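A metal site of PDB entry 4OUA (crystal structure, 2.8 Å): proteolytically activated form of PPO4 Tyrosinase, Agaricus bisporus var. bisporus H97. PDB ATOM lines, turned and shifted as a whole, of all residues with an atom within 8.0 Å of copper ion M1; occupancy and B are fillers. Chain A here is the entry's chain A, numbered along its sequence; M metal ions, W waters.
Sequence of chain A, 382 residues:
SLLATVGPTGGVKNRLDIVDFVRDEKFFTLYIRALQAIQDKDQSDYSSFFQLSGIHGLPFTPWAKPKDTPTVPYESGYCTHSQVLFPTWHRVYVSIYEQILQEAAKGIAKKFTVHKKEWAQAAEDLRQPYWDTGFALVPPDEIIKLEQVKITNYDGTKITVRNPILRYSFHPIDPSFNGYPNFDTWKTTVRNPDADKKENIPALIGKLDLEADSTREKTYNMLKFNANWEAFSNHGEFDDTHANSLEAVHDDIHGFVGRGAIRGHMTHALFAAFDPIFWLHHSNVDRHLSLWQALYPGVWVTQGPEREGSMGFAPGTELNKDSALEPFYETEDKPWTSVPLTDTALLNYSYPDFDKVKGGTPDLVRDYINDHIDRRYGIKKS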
ATOM      1  N   HIS A  56     -29.588   0.932  16.235  1.00  0.00           N
ATOM      2  CA  HIS A  56     -29.762   1.790  17.407  1.00  0.00           C
ATOM      3  C   HIS A  56     -30.315   3.165  17.028  1.00  0.00           C
ATOM      4  O   HIS A  56     -31.408   3.542  17.432  1.00  0.00           O
ATOM      5  CB  HIS A  56     -28.439   1.934  18.159  1.00  0.00           C
ATOM      6  CG  HIS A  56     -28.587   2.462  19.549  1.00  0.00           C
ATOM      7  ND1 HIS A  56     -28.379   3.791  19.870  1.00  0.00           N
ATOM      8  CD2 HIS A  56     -28.916   1.845  20.703  1.00  0.00           C
ATOM      9  CE1 HIS A  56     -28.568   3.965  21.164  1.00  0.00           C
ATOM     10  NE2 HIS A  56     -28.891   2.801  21.698  1.00  0.00           N
ATOM     11  N   GLY A  57     -29.549   3.909  16.235  1.00  0.00           N
ATOM     12  CA  GLY A  57     -29.952   5.244  15.816  1.00  0.00           C
ATOM     13  C   GLY A  57     -29.976   5.392  14.306  1.00  0.00           C
ATOM     14  O   GLY A  57     -30.705   4.666  13.621  1.00  0.00           O
ATOM     15  N   TYR A  78     -34.193   2.648  16.356  1.00  0.00           N
ATOM     16  CA  TYR A  78     -34.937   1.496  16.862  1.00  0.00           C
ATOM     17  C   TYR A  78     -34.902   1.448  18.386  1.00  0.00           C
ATOM     18  O   TYR A  78     -35.866   1.003  19.014  1.00  0.00           O
ATOM     19  CB  TYR A  78     -34.361   0.190  16.304  1.00  0.00           C
ATOM     20  CG  TYR A  78     -35.023  -0.306  15.039  1.00  0.00           C
ATOM     21  CD1 TYR A  78     -36.365  -0.678  15.033  1.00  0.00           C
ATOM     22  CD2 TYR A  78     -34.310  -0.436  13.861  1.00  0.00           C
ATOM     23  CE1 TYR A  78     -36.969  -1.146  13.881  1.00  0.00           C
ATOM     24  CE2 TYR A  78     -34.904  -0.897  12.703  1.00  0.00           C
ATOM     25  CZ  TYR A  78     -36.240  -1.255  12.721  1.00  0.00           C
ATOM     26  OH  TYR A  78     -36.832  -1.723  11.575  1.00  0.00           O
ATOM     27  N   CYS A  79     -33.796   1.899  18.964  1.00  0.00           N
ATOM     28  CA  CYS A  79     -33.557   1.766  20.395  1.00  0.00           C
ATOM     29  C   CYS A  79     -34.656   2.425  21.217  1.00  0.00           C
ATOM     30  O   CYS A  79     -35.131   3.502  20.894  1.00  0.00           O
ATOM     31  CB  CYS A  79     -32.190   2.349  20.781  1.00  0.00           C
ATOM     32  SG  CYS A  79     -32.062   4.147  20.635  1.00  0.00           S
ATOM     33  N   THR A  80     -35.050   1.746  22.288  1.00  0.00           N
ATOM     34  CA  THR A  80     -36.093   2.235  23.185  1.00  0.00           C
ATOM     35  C   THR A  80     -35.475   2.908  24.403  1.00  0.00           C
ATOM     36  O   THR A  80     -34.782   2.271  25.187  1.00  0.00           O
ATOM     37  CB  THR A  80     -37.019   1.093  23.631  1.00  0.00           C
ATOM     38  OG1 THR A  80     -36.236   0.105  24.323  1.00  0.00           O
ATOM     39  CG2 THR A  80     -37.695   0.450  22.440  1.00  0.00           C
ATOM     40  N   HIS A  81     -35.738   4.198  24.544  1.00  0.00           N
ATOM     41  CA  HIS A  81     -35.160   4.977  25.631  1.00  0.00           C
ATOM     42  C   HIS A  81     -36.232   5.782  26.351  1.00  0.00           C
ATOM     43  O   HIS A  81     -37.183   6.252  25.729  1.00  0.00           O
ATOM     44  CB  HIS A  81     -34.063   5.907  25.092  1.00  0.00           C
ATOM     45  CG  HIS A  81     -33.038   5.193  24.260  1.00  0.00           C
ATOM     46  ND1 HIS A  81     -32.978   5.319  22.888  1.00  0.00           N
ATOM     47  CD2 HIS A  81     -32.036   4.357  24.597  1.00  0.00           C
ATOM     48  CE1 HIS A  81     -31.979   4.583  22.419  1.00  0.00           C
ATOM     49  NE2 HIS A  81     -31.396   3.995  23.448  1.00  0.00           N
ATOM     50  N   PHE A  86     -36.819  -0.413  27.710  1.00  0.00           N
ATOM     51  CA  PHE A  86     -35.385  -0.172  27.575  1.00  0.00           C
ATOM     52  C   PHE A  86     -34.539  -1.402  27.863  1.00  0.00           C
ATOM     53  O   PHE A  86     -33.717  -1.805  27.029  1.00  0.00           O
ATOM     54  CB  PHE A  86     -34.950   0.969  28.499  1.00  0.00           C
ATOM     55  CG  PHE A  86     -33.454   1.133  28.582  1.00  0.00           C
ATOM     56  CD1 PHE A  86     -32.761   1.791  27.571  1.00  0.00           C
ATOM     57  CD2 PHE A  86     -32.741   0.634  29.657  1.00  0.00           C
ATOM     58  CE1 PHE A  86     -31.391   1.938  27.641  1.00  0.00           C
ATOM     59  CE2 PHE A  86     -31.375   0.781  29.736  1.00  0.00           C
ATOM     60  CZ  PHE A  86     -30.689   1.432  28.721  1.00  0.00           C
ATOM     61  N   TRP A  89     -35.361  -4.489  25.258  1.00  0.00           N
ATOM     62  CA  TRP A  89     -35.017  -4.209  23.868  1.00  0.00           C
ATOM     63  C   TRP A  89     -33.517  -4.311  23.641  1.00  0.00           C
ATOM     64  O   TRP A  89     -33.061  -4.765  22.586  1.00  0.00           O
ATOM     65  CB  TRP A  89     -35.510  -2.837  23.428  1.00  0.00           C
ATOM     66  CG  TRP A  89     -35.235  -2.541  21.985  1.00  0.00           C
ATOM     67  CD1 TRP A  89     -36.071  -2.739  20.928  1.00  0.00           C
ATOM     68  CD2 TRP A  89     -34.024  -2.004  21.433  1.00  0.00           C
ATOM     69  NE1 TRP A  89     -35.466  -2.364  19.754  1.00  0.00           N
ATOM     70  CE2 TRP A  89     -34.210  -1.907  20.037  1.00  0.00           C
ATOM     71  CE3 TRP A  89     -32.802  -1.591  21.977  1.00  0.00           C
ATOM     72  CZ2 TRP A  89     -33.221  -1.410  19.187  1.00  0.00           C
ATOM     73  CZ3 TRP A  89     -31.824  -1.101  21.133  1.00  0.00           C
ATOM     74  CH2 TRP A  89     -32.036  -1.017  19.759  1.00  0.00           C
ATOM     75  N   HIS A  90     -32.745  -3.879  24.628  1.00  0.00           N
ATOM     76  CA  HIS A  90     -31.296  -3.879  24.518  1.00  0.00           C
ATOM     77  C   HIS A  90     -30.707  -5.271  24.782  1.00  0.00           C
ATOM     78  O   HIS A  90     -29.631  -5.607  24.281  1.00  0.00           O
ATOM     79  CB  HIS A  90     -30.678  -2.849  25.463  1.00  0.00           C
ATOM     80  CG  HIS A  90     -30.893  -1.428  25.028  1.00  0.00           C
ATOM     81  ND1 HIS A  90     -32.120  -0.798  25.122  1.00  0.00           N
ATOM     82  CD2 HIS A  90     -30.054  -0.533  24.472  1.00  0.00           C
ATOM     83  CE1 HIS A  90     -32.012   0.430  24.653  1.00  0.00           C
ATOM     84  NE2 HIS A  90     -30.767   0.615  24.247  1.00  0.00           N
ATOM     85  N   TYR A  93     -30.901  -6.836  21.638  1.00  0.00           N
ATOM     86  CA  TYR A  93     -30.048  -6.060  20.741  1.00  0.00           C
ATOM     87  C   TYR A  93     -28.623  -6.588  20.745  1.00  0.00           C
ATOM     88  O   TYR A  93     -28.006  -6.763  19.690  1.00  0.00           O
ATOM     89  CB  TYR A  93     -30.059  -4.575  21.123  1.00  0.00           C
ATOM     90  CG  TYR A  93     -29.355  -3.676  20.132  1.00  0.00           C
ATOM     91  CD1 TYR A  93     -29.166  -4.070  18.811  1.00  0.00           C
ATOM     92  CD2 TYR A  93     -28.877  -2.432  20.522  1.00  0.00           C
ATOM     93  CE1 TYR A  93     -28.525  -3.246  17.903  1.00  0.00           C
ATOM     94  CE2 TYR A  93     -28.230  -1.601  19.618  1.00  0.00           C
ATOM     95  CZ  TYR A  93     -28.066  -2.007  18.319  1.00  0.00           C
ATOM     96  OH  TYR A  93     -27.423  -1.190  17.423  1.00  0.00           O
ATOM     97  N   GLU A 247     -31.285   2.589  33.374  1.00  0.00           N
ATOM     98  CA  GLU A 247     -30.915   3.446  32.244  1.00  0.00           C
ATOM     99  C   GLU A 247     -30.195   4.706  32.700  1.00  0.00           C
ATOM    100  O   GLU A 247     -29.248   5.150  32.042  1.00  0.00           O
ATOM    101  CB  GLU A 247     -32.156   3.822  31.437  1.00  0.00           C
ATOM    102  CG  GLU A 247     -31.857   4.636  30.188  1.00  0.00           C
ATOM    103  CD  GLU A 247     -33.112   5.035  29.429  1.00  0.00           C
ATOM    104  OE1 GLU A 247     -34.209   4.968  30.009  1.00  0.00           O
ATOM    105  OE2 GLU A 247     -32.991   5.416  28.243  1.00  0.00           O
ATOM    106  N   HIS A 250     -26.925   3.966  33.352  1.00  0.00           N
ATOM    107  CA  HIS A 250     -26.385   3.591  32.048  1.00  0.00           C
ATOM    108  C   HIS A 250     -25.979   4.819  31.231  1.00  0.00           C
ATOM    109  O   HIS A 250     -25.068   4.745  30.405  1.00  0.00           O
ATOM    110  CB  HIS A 250     -27.425   2.760  31.290  1.00  0.00           C
ATOM    111  CG  HIS A 250     -27.384   2.948  29.809  1.00  0.00           C
ATOM    112  ND1 HIS A 250     -28.192   3.859  29.152  1.00  0.00           N
ATOM    113  CD2 HIS A 250     -26.650   2.346  28.852  1.00  0.00           C
ATOM    114  CE1 HIS A 250     -27.946   3.804  27.859  1.00  0.00           C
ATOM    115  NE2 HIS A 250     -27.014   2.897  27.649  1.00  0.00           N
ATOM    116  N   ASP A 251     -26.653   5.931  31.464  1.00  0.00           N
ATOM    117  CA  ASP A 251     -26.406   7.158  30.707  1.00  0.00           C
ATOM    118  C   ASP A 251     -25.041   7.761  31.014  1.00  0.00           C
ATOM    119  O   ASP A 251     -24.419   8.359  30.137  1.00  0.00           O
ATOM    120  CB  ASP A 251     -27.501   8.191  30.992  1.00  0.00           C
ATOM    121  CG  ASP A 251     -28.860   7.754  30.474  1.00  0.00           C
ATOM    122  OD1 ASP A 251     -28.902   6.941  29.522  1.00  0.00           O
ATOM    123  OD2 ASP A 251     -29.878   8.237  31.008  1.00  0.00           O
ATOM    124  N   HIS A 254     -22.134   6.689  28.729  1.00  0.00           N
ATOM    125  CA  HIS A 254     -22.162   7.298  27.402  1.00  0.00           C
ATOM    126  C   HIS A 254     -21.573   8.705  27.455  1.00  0.00           C
ATOM    127  O   HIS A 254     -20.894   9.138  26.531  1.00  0.00           O
ATOM    128  CB  HIS A 254     -23.580   7.330  26.833  1.00  0.00           C
ATOM    129  CG  HIS A 254     -24.045   6.012  26.307  1.00  0.00           C
ATOM    130  ND1 HIS A 254     -23.566   5.464  25.145  1.00  0.00           N
ATOM    131  CD2 HIS A 254     -24.963   5.139  26.782  1.00  0.00           C
ATOM    132  CE1 HIS A 254     -24.160   4.303  24.929  1.00  0.00           C
ATOM    133  NE2 HIS A 254     -25.016   4.073  25.909  1.00  0.00           N
ATOM    134  N   ALA A 269     -27.230   9.493  20.990  1.00  0.00           N
ATOM    135  CA  ALA A 269     -27.980   8.265  20.771  1.00  0.00           C
ATOM    136  C   ALA A 269     -28.049   7.862  19.300  1.00  0.00           C
ATOM    137  O   ALA A 269     -28.289   6.697  18.971  1.00  0.00           O
ATOM    138  CB  ALA A 269     -29.378   8.405  21.340  1.00  0.00           C
ATOM    139  N   ALA A 272     -24.112   6.578  18.908  1.00  0.00           N
ATOM    140  CA  ALA A 272     -23.444   5.869  20.001  1.00  0.00           C
ATOM    141  C   ALA A 272     -23.136   4.412  19.666  1.00  0.00           C
ATOM    142  O   ALA A 272     -22.102   3.887  20.086  1.00  0.00           O
ATOM    143  CB  ALA A 272     -24.296   5.941  21.260  1.00  0.00           C
ATOM    144  N   ALA A 273     -24.017   3.774  18.910  1.00  0.00           N
ATOM    145  CA  ALA A 273     -23.869   2.364  18.588  1.00  0.00           C
ATOM    146  C   ALA A 273     -22.651   2.090  17.711  1.00  0.00           C
ATOM    147  O   ALA A 273     -22.071   0.999  17.753  1.00  0.00           O
ATOM    148  CB  ALA A 273     -25.132   1.844  17.908  1.00  0.00           C
ATOM    149  N   PHE A 278     -19.481   0.436  22.651  1.00  0.00           N
ATOM    150  CA  PHE A 278     -20.909   0.466  22.956  1.00  0.00           C
ATOM    151  C   PHE A 278     -21.425  -0.899  23.376  1.00  0.00           C
ATOM    152  O   PHE A 278     -22.315  -1.010  24.216  1.00  0.00           O
ATOM    153  CB  PHE A 278     -21.689   0.986  21.740  1.00  0.00           C
ATOM    154  CG  PHE A 278     -23.180   0.860  21.868  1.00  0.00           C
ATOM    155  CD1 PHE A 278     -23.929   1.894  22.399  1.00  0.00           C
ATOM    156  CD2 PHE A 278     -23.834  -0.281  21.426  1.00  0.00           C
ATOM    157  CE1 PHE A 278     -25.304   1.793  22.513  1.00  0.00           C
ATOM    158  CE2 PHE A 278     -25.206  -0.397  21.531  1.00  0.00           C
ATOM    159  CZ  PHE A 278     -25.939   0.644  22.080  1.00  0.00           C
ATOM    160  N   HIS A 282     -23.204  -2.251  26.979  1.00  0.00           N
ATOM    161  CA  HIS A 282     -24.551  -2.798  27.095  1.00  0.00           C
ATOM    162  C   HIS A 282     -24.563  -4.301  27.341  1.00  0.00           C
ATOM    163  O   HIS A 282     -25.612  -4.875  27.639  1.00  0.00           O
ATOM    164  CB  HIS A 282     -25.359  -2.441  25.849  1.00  0.00           C
ATOM    165  CG  HIS A 282     -25.866  -1.040  25.832  1.00  0.00           C
ATOM    166  ND1 HIS A 282     -27.135  -0.701  26.245  1.00  0.00           N
ATOM    167  CD2 HIS A 282     -25.259   0.119  25.493  1.00  0.00           C
ATOM    168  CE1 HIS A 282     -27.304   0.604  26.131  1.00  0.00           C
ATOM    169  NE2 HIS A 282     -26.173   1.131  25.686  1.00  0.00           N
HETATM  170 CU    CU M   1     -30.083   2.357  23.322  1.00  0.00          CU
HETATM  171 CU    CU M   2     -26.699   3.028  25.700  1.00  0.00          CU
HETATM  172  O   HOH W   1     -28.470   3.738  24.468  1.00  0.00           O
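The backbone carbonyl oxygen (O) of Phe 86 sits at hydrogen-bond distance from a ring nitrogen (ND1) of His 90, 2.7 Å away. CE1 of His 81 is covalently linked to SG of Cys 79. The backbone carbonyl oxygen (O) of His 56 lies within hydrogen-bond range of the backbone NH (N) of Tyr 78 (3.1 Å). The backbone NH (N) of His 56 sits at hydrogen-bond distance from the side-chain hydroxyl (OH) of Tyr 93 (3.3 Å). ND1 of His 56 lies within hydrogen-bond range of O of Ala 269 (3.0 Å). The backbone NH (N) of Cys 79 lies within hydrogen-bond range of the backbone carbonyl oxygen (O) of His 56, 3.3 Å away.
Cys 79 touches copper ion M1. Four residues have an atom within 4 Å of copper ion M1: His 56, Cys 79, His 81 and His 90. The nearest printed residue that does not touch copper ion M1 is His 282 (4.3 Å).
Copper ion M1 is bound by a ring nitrogen (NE2) of His 56 (2.1 Å), a ring nitrogen (NE2) of His 90 (2.1 Å), a ring nitrogen (NE2) of His 81 (2.1 Å) and water W1 (2.4 Å).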
